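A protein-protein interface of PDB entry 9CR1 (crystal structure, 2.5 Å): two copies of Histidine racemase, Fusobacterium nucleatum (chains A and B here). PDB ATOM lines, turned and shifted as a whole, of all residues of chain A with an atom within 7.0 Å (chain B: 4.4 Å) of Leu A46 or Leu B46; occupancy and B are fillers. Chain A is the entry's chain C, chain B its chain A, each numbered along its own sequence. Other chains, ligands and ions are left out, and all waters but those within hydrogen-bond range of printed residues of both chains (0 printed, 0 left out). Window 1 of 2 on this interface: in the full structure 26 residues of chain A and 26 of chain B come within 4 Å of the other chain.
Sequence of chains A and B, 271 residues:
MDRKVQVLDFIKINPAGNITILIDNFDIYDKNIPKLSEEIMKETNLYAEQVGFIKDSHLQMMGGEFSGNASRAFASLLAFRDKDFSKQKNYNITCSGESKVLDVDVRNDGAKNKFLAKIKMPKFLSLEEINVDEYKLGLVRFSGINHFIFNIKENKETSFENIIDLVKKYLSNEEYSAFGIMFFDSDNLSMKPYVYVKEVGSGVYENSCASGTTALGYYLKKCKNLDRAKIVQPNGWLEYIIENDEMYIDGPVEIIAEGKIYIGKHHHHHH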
ATOM      1  N   PHE A  10      15.146  -4.545  -3.795  1.00  0.00           N
ATOM      2  CA  PHE A  10      15.518  -3.294  -3.152  1.00  0.00           C
ATOM      3  C   PHE A  10      14.624  -2.155  -3.624  1.00  0.00           C
ATOM      4  O   PHE A  10      14.104  -2.170  -4.743  1.00  0.00           O
ATOM      5  CB  PHE A  10      17.000  -2.949  -3.437  1.00  0.00           C
ATOM      6  CG  PHE A  10      17.210  -2.111  -4.675  1.00  0.00           C
ATOM      7  CD1 PHE A  10      17.148  -0.727  -4.613  1.00  0.00           C
ATOM      8  CD2 PHE A  10      17.479  -2.705  -5.896  1.00  0.00           C
ATOM      9  CE1 PHE A  10      17.338   0.042  -5.741  1.00  0.00           C
ATOM     10  CE2 PHE A  10      17.673  -1.939  -7.031  1.00  0.00           C
ATOM     11  CZ  PHE A  10      17.600  -0.563  -6.950  1.00  0.00           C
ATOM     12  N   ILE A  11      14.457  -1.165  -2.752  1.00  0.00           N
ATOM     13  CA  ILE A  11      13.782   0.087  -3.068  1.00  0.00           C
ATOM     14  C   ILE A  11      14.639   1.206  -2.499  1.00  0.00           C
ATOM     15  O   ILE A  11      14.926   1.216  -1.294  1.00  0.00           O
ATOM     16  CB  ILE A  11      12.362   0.146  -2.484  1.00  0.00           C
ATOM     17  CG1 ILE A  11      11.524  -1.038  -2.961  1.00  0.00           C
ATOM     18  CG2 ILE A  11      11.681   1.456  -2.876  1.00  0.00           C
ATOM     19  CD1 ILE A  11      11.304  -2.094  -1.899  1.00  0.00           C
ATOM     20  N   LYS A  12      15.055   2.137  -3.353  1.00  0.00           N
ATOM     21  CA  LYS A  12      15.856   3.276  -2.920  1.00  0.00           C
ATOM     22  C   LYS A  12      14.958   4.502  -2.819  1.00  0.00           C
ATOM     23  O   LYS A  12      14.326   4.897  -3.805  1.00  0.00           O
ATOM     24  CB  LYS A  12      17.018   3.555  -3.871  1.00  0.00           C
ATOM     25  CG  LYS A  12      17.827   4.783  -3.451  1.00  0.00           C
ATOM     26  CD  LYS A  12      19.249   4.731  -3.973  1.00  0.00           C
ATOM     27  CE  LYS A  12      20.236   5.341  -2.985  1.00  0.00           C
ATOM     28  NZ  LYS A  12      21.609   5.361  -3.569  1.00  0.00           N
ATOM     29  N   ILE A  21      17.462   2.470   1.989  1.00  0.00           N
ATOM     30  CA  ILE A  21      17.246   1.288   1.163  1.00  0.00           C
ATOM     31  C   ILE A  21      16.349   0.341   1.957  1.00  0.00           C
ATOM     32  O   ILE A  21      16.680  -0.029   3.094  1.00  0.00           O
ATOM     33  CB  ILE A  21      18.563   0.594   0.777  1.00  0.00           C
ATOM     34  CG1 ILE A  21      19.431   1.484  -0.129  1.00  0.00           C
ATOM     35  CG2 ILE A  21      18.282  -0.747   0.099  1.00  0.00           C
ATOM     36  CD1 ILE A  21      18.692   2.215  -1.242  1.00  0.00           C
ATOM     37  N   ILE A  23      14.662  -3.423   1.853  1.00  0.00           N
ATOM     38  CA  ILE A  23      14.722  -4.745   1.241  1.00  0.00           C
ATOM     39  C   ILE A  23      13.373  -5.422   1.435  1.00  0.00           C
ATOM     40  O   ILE A  23      12.798  -5.387   2.533  1.00  0.00           O
ATOM     41  CB  ILE A  23      15.857  -5.597   1.839  1.00  0.00           C
ATOM     42  CG1 ILE A  23      17.196  -4.862   1.741  1.00  0.00           C
ATOM     43  CG2 ILE A  23      15.939  -6.944   1.126  1.00  0.00           C
ATOM     44  CD1 ILE A  23      17.394  -4.071   0.459  1.00  0.00           C
ATOM     45  N   GLU A  39      27.312  -3.778   3.734  1.00  0.00           N
ATOM     46  CA  GLU A  39      27.801  -3.789   2.358  1.00  0.00           C
ATOM     47  C   GLU A  39      26.885  -2.986   1.440  1.00  0.00           C
ATOM     48  O   GLU A  39      27.358  -2.296   0.531  1.00  0.00           O
ATOM     49  CB  GLU A  39      27.930  -5.225   1.854  1.00  0.00           C
ATOM     50  CG  GLU A  39      29.296  -5.556   1.260  1.00  0.00           C
ATOM     51  CD  GLU A  39      29.428  -7.019   0.863  1.00  0.00           C
ATOM     52  OE1 GLU A  39      28.929  -7.396  -0.220  1.00  0.00           O
ATOM     53  OE2 GLU A  39      30.035  -7.794   1.634  1.00  0.00           O
ATOM     54  N   ILE A  40      25.572  -3.060   1.665  1.00  0.00           N
ATOM     55  CA  ILE A  40      24.637  -2.345   0.805  1.00  0.00           C
ATOM     56  C   ILE A  40      24.811  -0.840   0.942  1.00  0.00           C
ATOM     57  O   ILE A  40      24.463  -0.091   0.028  1.00  0.00           O
ATOM     58  CB  ILE A  40      23.187  -2.765   1.118  1.00  0.00           C
ATOM     59  CG1 ILE A  40      22.932  -4.196   0.626  1.00  0.00           C
ATOM     60  CG2 ILE A  40      22.187  -1.789   0.493  1.00  0.00           C
ATOM     61  CD1 ILE A  40      21.477  -4.672   0.790  1.00  0.00           C
ATOM     62  N   MET A  41      25.328  -0.368   2.078  1.00  0.00           N
ATOM     63  CA  MET A  41      25.411   1.068   2.325  1.00  0.00           C
ATOM     64  C   MET A  41      26.651   1.708   1.712  1.00  0.00           C
ATOM     65  O   MET A  41      26.692   2.936   1.567  1.00  0.00           O
ATOM     66  CB  MET A  41      25.383   1.340   3.837  1.00  0.00           C
ATOM     67  CG  MET A  41      23.994   1.590   4.398  1.00  0.00           C
ATOM     68  SD  MET A  41      23.885   1.710   6.208  1.00  0.00           S
ATOM     69  CE  MET A  41      25.129   0.531   6.745  1.00  0.00           C
ATOM     70  N   LYS A  42      27.649   0.915   1.335  1.00  0.00           N
ATOM     71  CA  LYS A  42      28.891   1.483   0.835  1.00  0.00           C
ATOM     72  C   LYS A  42      28.644   2.350  -0.397  1.00  0.00           C
ATOM     73  O   LYS A  42      27.661   2.177  -1.125  1.00  0.00           O
ATOM     74  CB  LYS A  42      29.884   0.376   0.487  1.00  0.00           C
ATOM     75  CG  LYS A  42      30.388  -0.418   1.672  1.00  0.00           C
ATOM     76  CD  LYS A  42      31.365  -1.488   1.216  1.00  0.00           C
ATOM     77  CE  LYS A  42      31.684  -2.473   2.330  1.00  0.00           C
ATOM     78  NZ  LYS A  42      32.995  -3.152   2.091  1.00  0.00           N
ATOM     79  N   GLU A  43      29.556   3.306  -0.611  1.00  0.00           N
ATOM     80  CA  GLU A  43      29.557   4.089  -1.841  1.00  0.00           C
ATOM     81  C   GLU A  43      29.964   3.234  -3.034  1.00  0.00           C
ATOM     82  O   GLU A  43      29.538   3.508  -4.162  1.00  0.00           O
ATOM     83  CB  GLU A  43      30.501   5.288  -1.693  1.00  0.00           C
ATOM     84  CG  GLU A  43      30.494   6.274  -2.867  1.00  0.00           C
ATOM     85  CD  GLU A  43      31.898   6.713  -3.299  1.00  0.00           C
ATOM     86  OE1 GLU A  43      32.893   6.150  -2.797  1.00  0.00           O
ATOM     87  OE2 GLU A  43      32.018   7.620  -4.157  1.00  0.00           O
ATOM     88  N   THR A  44      30.792   2.208  -2.809  1.00  0.00           N
ATOM     89  CA  THR A  44      31.152   1.240  -3.843  1.00  0.00           C
ATOM     90  C   THR A  44      30.041   0.228  -4.112  1.00  0.00           C
ATOM     91  O   THR A  44      30.225  -0.668  -4.941  1.00  0.00           O
ATOM     92  CB  THR A  44      32.444   0.509  -3.451  1.00  0.00           C
ATOM     93  OG1 THR A  44      32.320  -0.079  -2.150  1.00  0.00           O
ATOM     94  CG2 THR A  44      33.613   1.478  -3.417  1.00  0.00           C
ATOM     95  N   ASN A  45      28.895   0.355  -3.441  1.00  0.00           N
ATOM     96  CA  ASN A  45      27.706  -0.460  -3.687  1.00  0.00           C
ATOM     97  C   ASN A  45      26.560   0.476  -4.068  1.00  0.00           C
ATOM     98  O   ASN A  45      26.796   1.629  -4.447  1.00  0.00           O
ATOM     99  CB  ASN A  45      27.346  -1.281  -2.446  1.00  0.00           C
ATOM    100  CG  ASN A  45      26.646  -2.591  -2.792  1.00  0.00           C
ATOM    101  OD1 ASN A  45      25.413  -2.674  -2.780  1.00  0.00           O
ATOM    102  ND2 ASN A  45      27.431  -3.628  -3.083  1.00  0.00           N
ATOM    103  N   LEU A  46      25.320   0.002  -3.982  1.00  0.00           N
ATOM    104  CA  LEU A  46      24.190   0.920  -3.924  1.00  0.00           C
ATOM    105  C   LEU A  46      24.407   1.843  -2.737  1.00  0.00           C
ATOM    106  O   LEU A  46      24.717   1.382  -1.639  1.00  0.00           O
ATOM    107  CB  LEU A  46      22.882   0.151  -3.773  1.00  0.00           C
ATOM    108  CG  LEU A  46      21.633   0.804  -4.373  1.00  0.00           C
ATOM    109  CD1 LEU A  46      21.738   0.879  -5.893  1.00  0.00           C
ATOM    110  CD2 LEU A  46      20.369   0.059  -3.963  1.00  0.00           C
ATOM    111  N   TYR A  47      24.284   3.146  -2.937  1.00  0.00           N
ATOM    112  CA  TYR A  47      24.561   4.055  -1.826  1.00  0.00           C
ATOM    113  C   TYR A  47      23.351   4.148  -0.903  1.00  0.00           C
ATOM    114  O   TYR A  47      22.204   4.010  -1.336  1.00  0.00           O
ATOM    115  CB  TYR A  47      24.946   5.438  -2.336  1.00  0.00           C
ATOM    116  CG  TYR A  47      25.856   6.212  -1.400  1.00  0.00           C
ATOM    117  CD1 TYR A  47      26.603   5.570  -0.415  1.00  0.00           C
ATOM    118  CD2 TYR A  47      25.970   7.593  -1.505  1.00  0.00           C
ATOM    119  CE1 TYR A  47      27.429   6.279   0.436  1.00  0.00           C
ATOM    120  CE2 TYR A  47      26.798   8.312  -0.660  1.00  0.00           C
ATOM    121  CZ  TYR A  47      27.526   7.649   0.307  1.00  0.00           C
ATOM    122  OH  TYR A  47      28.353   8.357   1.149  1.00  0.00           O
ATOM    123  N   ALA A  48      23.619   4.376   0.382  1.00  0.00           N
ATOM    124  CA  ALA A  48      22.564   4.454   1.383  1.00  0.00           C
ATOM    125  C   ALA A  48      23.138   4.973   2.692  1.00  0.00           C
ATOM    126  O   ALA A  48      24.312   4.753   3.001  1.00  0.00           O
ATOM    127  CB  ALA A  48      21.910   3.086   1.622  1.00  0.00           C
ATOM    128  N   ILE A 256      13.256   6.751  -5.559  1.00  0.00           N
ATOM    129  CA  ILE A 256      14.346   6.916  -6.513  1.00  0.00           C
ATOM    130  C   ILE A 256      14.391   5.765  -7.508  1.00  0.00           C
ATOM    131  O   ILE A 256      14.406   5.980  -8.724  1.00  0.00           O
ATOM    132  CB  ILE A 256      15.687   7.060  -5.758  1.00  0.00           C
ATOM    133  CG1 ILE A 256      15.805   8.453  -5.135  1.00  0.00           C
ATOM    134  CG2 ILE A 256      16.859   6.788  -6.696  1.00  0.00           C
ATOM    135  CD1 ILE A 256      16.832   8.535  -4.022  1.00  0.00           C
ATOM    136  N   ALA A 257      14.422   4.530  -7.012  1.00  0.00           N
ATOM    137  CA  ALA A 257      14.614   3.377  -7.877  1.00  0.00           C
ATOM    138  C   ALA A 257      14.210   2.120  -7.125  1.00  0.00           C
ATOM    139  O   ALA A 257      14.025   2.129  -5.907  1.00  0.00           O
ATOM    140  CB  ALA A 257      16.067   3.285  -8.354  1.00  0.00           C
ATOM    141  N   GLU A 258      14.070   1.032  -7.876  1.00  0.00           N
ATOM    142  CA  GLU A 258      13.758  -0.264  -7.293  1.00  0.00           C
ATOM    143  C   GLU A 258      14.107  -1.343  -8.303  1.00  0.00           C
ATOM    144  O   GLU A 258      14.145  -1.099  -9.512  1.00  0.00           O
ATOM    145  CB  GLU A 258      12.285  -0.357  -6.877  1.00  0.00           C
ATOM    146  CG  GLU A 258      11.320  -0.653  -8.010  1.00  0.00           C
ATOM    147  CD  GLU A 258       9.871  -0.675  -7.544  1.00  0.00           C
ATOM    148  OE1 GLU A 258       9.528  -1.508  -6.666  1.00  0.00           O
ATOM    149  OE2 GLU A 258       9.075   0.145  -8.053  1.00  0.00           O
ATOM    150  N   LYS A 260      16.609  -5.158  -8.380  1.00  0.00           N
ATOM    151  CA  LYS A 260      17.383  -6.243  -7.802  1.00  0.00           C
ATOM    152  C   LYS A 260      18.772  -5.749  -7.432  1.00  0.00           C
ATOM    153  O   LYS A 260      19.307  -4.828  -8.051  1.00  0.00           O
ATOM    154  CB  LYS A 260      17.489  -7.419  -8.780  1.00  0.00           C
ATOM    155  CG  LYS A 260      16.147  -8.028  -9.162  1.00  0.00           C
ATOM    156  CD  LYS A 260      15.573  -8.871  -8.032  1.00  0.00           C
ATOM    157  CE  LYS A 260      14.169  -9.373  -8.358  1.00  0.00           C
ATOM    158  NZ  LYS A 260      13.110  -8.595  -7.641  1.00  0.00           N
ATOM    159  N   ILE A 261      19.351  -6.368  -6.410  1.00  0.00           N
ATOM    160  CA  ILE A 261      20.710  -6.081  -5.971  1.00  0.00           C
ATOM    161  C   ILE A 261      21.419  -7.410  -5.754  1.00  0.00           C
ATOM    162  O   ILE A 261      20.825  -8.364  -5.240  1.00  0.00           O
ATOM    163  CB  ILE A 261      20.725  -5.219  -4.691  1.00  0.00           C
ATOM    164  CG1 ILE A 261      22.122  -5.183  -4.079  1.00  0.00           C
ATOM    165  CG2 ILE A 261      19.718  -5.743  -3.689  1.00  0.00           C
ATOM    166  CD1 ILE A 261      22.303  -4.109  -3.037  1.00  0.00           C
ATOM    167  N   PHE B  10      18.139   0.761 -15.656  1.00  0.00           N
ATOM    168  CA  PHE B  10      19.470   1.048 -15.155  1.00  0.00           C
ATOM    169  C   PHE B  10      20.196  -0.236 -14.787  1.00  0.00           C
ATOM    170  O   PHE B  10      19.580  -1.256 -14.474  1.00  0.00           O
ATOM    171  CB  PHE B  10      19.416   1.987 -13.922  1.00  0.00           C
ATOM    172  CG  PHE B  10      19.296   1.261 -12.601  1.00  0.00           C
ATOM    173  CD1 PHE B  10      20.430   0.844 -11.915  1.00  0.00           C
ATOM    174  CD2 PHE B  10      18.049   1.007 -12.040  1.00  0.00           C
ATOM    175  CE1 PHE B  10      20.323   0.175 -10.707  1.00  0.00           C
ATOM    176  CE2 PHE B  10      17.933   0.338 -10.829  1.00  0.00           C
ATOM    177  CZ  PHE B  10      19.074  -0.077 -10.163  1.00  0.00           C
ATOM    178  N   LYS B  12      23.711  -0.711 -12.284  1.00  0.00           N
ATOM    179  CA  LYS B  12      24.775  -0.096 -11.504  1.00  0.00           C
ATOM    180  C   LYS B  12      25.920  -1.087 -11.383  1.00  0.00           C
ATOM    181  O   LYS B  12      25.701  -2.261 -11.063  1.00  0.00           O
ATOM    182  CB  LYS B  12      24.285   0.319 -10.120  1.00  0.00           C
ATOM    183  CG  LYS B  12      25.203   1.312  -9.431  1.00  0.00           C
ATOM    184  CD  LYS B  12      24.467   2.097  -8.353  1.00  0.00           C
ATOM    185  CE  LYS B  12      25.419   2.543  -7.249  1.00  0.00           C
ATOM    186  NZ  LYS B  12      25.125   3.923  -6.775  1.00  0.00           N
ATOM    187  N   ILE B  21      26.749   3.890 -13.891  1.00  0.00           N
ATOM    188  CA  ILE B  21      25.376   3.485 -14.162  1.00  0.00           C
ATOM    189  C   ILE B  21      25.200   3.458 -15.674  1.00  0.00           C
ATOM    190  O   ILE B  21      25.602   4.401 -16.366  1.00  0.00           O
ATOM    191  CB  ILE B  21      24.353   4.433 -13.514  1.00  0.00           C
ATOM    192  CG1 ILE B  21      24.523   4.461 -11.994  1.00  0.00           C
ATOM    193  CG2 ILE B  21      22.934   4.000 -13.868  1.00  0.00           C
ATOM    194  CD1 ILE B  21      23.731   5.555 -11.320  1.00  0.00           C
ATOM    195  N   ILE B  40      20.875  11.444 -12.336  1.00  0.00           N
ATOM    196  CA  ILE B  40      21.112  10.050 -11.995  1.00  0.00           C
ATOM    197  C   ILE B  40      22.293   9.897 -11.042  1.00  0.00           C
ATOM    198  O   ILE B  40      22.380   8.893 -10.331  1.00  0.00           O
ATOM    199  CB  ILE B  40      21.334   9.229 -13.288  1.00  0.00           C
ATOM    200  CG1 ILE B  40      20.076   9.212 -14.174  1.00  0.00           C
ATOM    201  CG2 ILE B  40      21.777   7.792 -12.973  1.00  0.00           C
ATOM    202  CD1 ILE B  40      18.768   9.391 -13.446  1.00  0.00           C
ATOM    203  N   MET B  41      23.210  10.871 -11.006  1.00  0.00           N
ATOM    204  CA  MET B  41      24.467  10.711 -10.283  1.00  0.00           C
ATOM    205  C   MET B  41      24.458  11.287  -8.872  1.00  0.00           C
ATOM    206  O   MET B  41      25.292  10.881  -8.055  1.00  0.00           O
ATOM    207  CB  MET B  41      25.614  11.384 -11.047  1.00  0.00           C
ATOM    208  CG  MET B  41      26.030  10.704 -12.331  1.00  0.00           C
ATOM    209  SD  MET B  41      26.880  11.878 -13.389  1.00  0.00           S
ATOM    210  CE  MET B  41      28.579  11.639 -12.865  1.00  0.00           C
ATOM    211  N   LYS B  42      23.566  12.230  -8.575  1.00  0.00           N
ATOM    212  CA  LYS B  42      23.566  12.881  -7.276  1.00  0.00           C
ATOM    213  C   LYS B  42      23.413  11.855  -6.154  1.00  0.00           C
ATOM    214  O   LYS B  42      22.919  10.737  -6.351  1.00  0.00           O
ATOM    215  CB  LYS B  42      22.432  13.904  -7.191  1.00  0.00           C
ATOM    216  CG  LYS B  42      22.820  15.359  -7.481  1.00  0.00           C
ATOM    217  CD  LYS B  42      24.030  15.857  -6.669  1.00  0.00           C
ATOM    218  CE  LYS B  42      23.781  15.836  -5.165  1.00  0.00           C
ATOM    219  NZ  LYS B  42      23.109  17.076  -4.688  1.00  0.00           N
ATOM    220  N   ASN B  45      19.894  10.747  -5.363  1.00  0.00           N
ATOM    221  CA  ASN B  45      19.325   9.779  -6.296  1.00  0.00           C
ATOM    222  C   ASN B  45      20.188   8.525  -6.172  1.00  0.00           C
ATOM    223  O   ASN B  45      20.816   8.289  -5.132  1.00  0.00           O
ATOM    224  CB  ASN B  45      19.275  10.374  -7.711  1.00  0.00           C
ATOM    225  CG  ASN B  45      18.172   9.773  -8.556  1.00  0.00           C
ATOM    226  OD1 ASN B  45      18.430   8.943  -9.421  1.00  0.00           O
ATOM    227  ND2 ASN B  45      16.934  10.183  -8.304  1.00  0.00           N
ATOM    228  N   LEU B  46      20.231   7.696  -7.217  1.00  0.00           N
ATOM    229  CA  LEU B  46      21.277   6.681  -7.284  1.00  0.00           C
ATOM    230  C   LEU B  46      22.618   7.402  -7.377  1.00  0.00           C
ATOM    231  O   LEU B  46      22.758   8.384  -8.109  1.00  0.00           O
ATOM    232  CB  LEU B  46      21.076   5.753  -8.481  1.00  0.00           C
ATOM    233  CG  LEU B  46      21.137   4.243  -8.217  1.00  0.00           C
ATOM    234  CD1 LEU B  46      20.084   3.834  -7.180  1.00  0.00           C
ATOM    235  CD2 LEU B  46      20.929   3.425  -9.491  1.00  0.00           C
ATOM    236  N   TYR B  47      23.593   6.956  -6.596  1.00  0.00           N
ATOM    237  CA  TYR B  47      24.911   7.578  -6.674  1.00  0.00           C
ATOM    238  C   TYR B  47      25.634   7.100  -7.929  1.00  0.00           C
ATOM    239  O   TYR B  47      25.318   6.051  -8.488  1.00  0.00           O
ATOM    240  CB  TYR B  47      25.726   7.270  -5.417  1.00  0.00           C
ATOM    241  CG  TYR B  47      27.056   7.976  -5.374  1.00  0.00           C
ATOM    242  CD1 TYR B  47      27.127   9.355  -5.261  1.00  0.00           C
ATOM    243  CD2 TYR B  47      28.240   7.261  -5.464  1.00  0.00           C
ATOM    244  CE1 TYR B  47      28.348  10.006  -5.231  1.00  0.00           C
ATOM    245  CE2 TYR B  47      29.467   7.901  -5.441  1.00  0.00           C
ATOM    246  CZ  TYR B  47      29.518   9.272  -5.322  1.00  0.00           C
ATOM    247  OH  TYR B  47      30.748   9.899  -5.300  1.00  0.00           O
ATOM    248  N   ALA B  48      26.603   7.899  -8.381  1.00  0.00           N
ATOM    249  CA  ALA B  48      27.413   7.532  -9.536  1.00  0.00           C
ATOM    250  C   ALA B  48      28.532   8.530  -9.802  1.00  0.00           C
ATOM    251  O   ALA B  48      28.346   9.742  -9.639  1.00  0.00           O
ATOM    252  CB  ALA B  48      26.540   7.407 -10.791  1.00  0.00           C
ATOM    253  N   ILE B 256      26.385  -4.353  -9.411  1.00  0.00           N
ATOM    254  CA  ILE B 256      25.799  -4.037  -8.114  1.00  0.00           C
ATOM    255  C   ILE B 256      24.312  -4.354  -8.123  1.00  0.00           C
ATOM    256  O   ILE B 256      23.850  -5.248  -7.405  1.00  0.00           O
ATOM    257  CB  ILE B 256      26.031  -2.557  -7.754  1.00  0.00           C
ATOM    258  CG1 ILE B 256      27.482  -2.325  -7.344  1.00  0.00           C
ATOM    259  CG2 ILE B 256      25.091  -2.106  -6.633  1.00  0.00           C
ATOM    260  CD1 ILE B 256      28.002  -0.977  -7.755  1.00  0.00           C
ATOM    261  N   ALA B 257      23.552  -3.605  -8.919  1.00  0.00           N
ATOM    262  CA  ALA B 257      22.101  -3.661  -8.864  1.00  0.00           C
ATOM    263  C   ALA B 257      21.532  -3.423 -10.253  1.00  0.00           C
ATOM    264  O   ALA B 257      22.224  -2.957 -11.163  1.00  0.00           O
ATOM    265  CB  ALA B 257      21.548  -2.630  -7.874  1.00  0.00           C
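Leu A46 touches just these residues of chain B: Lys B12, Leu B46 and Ile B256. Of chain A, only Lys A12 (3.4 Å), Leu A46 (3.6 Å) and Ile A256 (3.5 Å) come within 4 Å of Leu B46. Printed residues of chain B within 4 Å of Asn A45: Lys B12 (3.3 Å) and Ile B256 (3.9 Å). Of the printed residues of chain B, Lys A260 touches Ala B257. Printed residues of chain A within 4 Å of Lys B12: Asn A45 and Leu A46. Printed residues of chain A within 4 Å of Phe B10: Phe A10. The nearest residue of chain A that does not touch Leu B46 is Ala A257 (4.2 Å).
Phe A10 touches its own counterpart, Phe B10. Lys A12 touches Asn B45, and with the chains exchanged Asn A45 touches Lys B12. Leu A46 touches Ile B256, and with the chains exchanged Ile A256 touches Leu B46. Tyr B47 touches its own counterpart, Tyr A47.
The side-chain carboxylate (OE2) of Glu A43 is in hydrogen-bond range of the side-chain hydroxyl (OH) of Tyr B47 (2.8 Å). The backbone carbonyl oxygen of Asn B45 is in hydrogen-bond range of the side-chain amino group of Lys A12 (3.4 Å).
Of the 12 printed residues of chain B, 7 touch a printed residue of chain A. Printed residues of chain B that touch a printed residue of chain A: Phe B10, Lys B12, Asn B45, Leu B46, Tyr B47, Ile B256 and Ala B257. Hydrophobic or aromatic side chains of chain B within 4 Å of the printed part of chain A: Phe B10, Leu B46, Tyr B47, Ile B256 and Ala B257. Printed residues of chain A that touch a printed residue of chain B: Phe A10, Lys A12, Glu A43, Thr A44, Asn A45, Leu A46, Tyr A47, Ile A256, Lys A260 and Ile A261. Hydrophobic or aromatic side chains of chain A within 4 Å of the printed part of chain B: Phe A10, Leu A46, Tyr A47, Ile A256 and Ile A261. Among the printed residues, 16 pairs touch across the chains. Among the printed residues, no Asp or Glu carboxylate lies within 4 Å of a Lys or Arg side-chain nitrogen of the other chain.
Among the printed residues, merely in contact across the chains: Phe A10 with Phe B10, Lys A12 with Leu B46, Lys A12 with Tyr B47, Thr A44 with Ile B256, Asn A45 with Lys B12, Asn A45 with Ile B256, Leu A46 with Lys B12, Leu A46 with Leu B46, Leu A46 with Ile B256, Tyr A47 with Tyr B47, Ile A256 with Asn B45, Ile A256 with Leu B46, Lys A260 with Ala B257 and Ile A261 with Ile B256.
The backbone carbonyl oxygen of Lys A12 lies within hydrogen-bond range of the backbone NH of Ile A256, 2.8 Å away. O of Ala B257 sits at hydrogen-bond distance from N of Lys B12 (2.9 Å). The backbone NH of Lys A12 is in hydrogen-bond range of the backbone carbonyl oxygen of Ala A257 (2.8 Å). O of Lys B12 is in hydrogen-bond range of N of Ile B256 (2.8 Å). The backbone carbonyl oxygen (O) of Tyr A47 sits at hydrogen-bond distance from the side-chain amino group (NZ) of Lys A12 (2.7 Å). The backbone carbonyl oxygen (O) of Tyr B47 lies within hydrogen-bond range of the side-chain amino group (NZ) of Lys B12 (2.7 Å).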
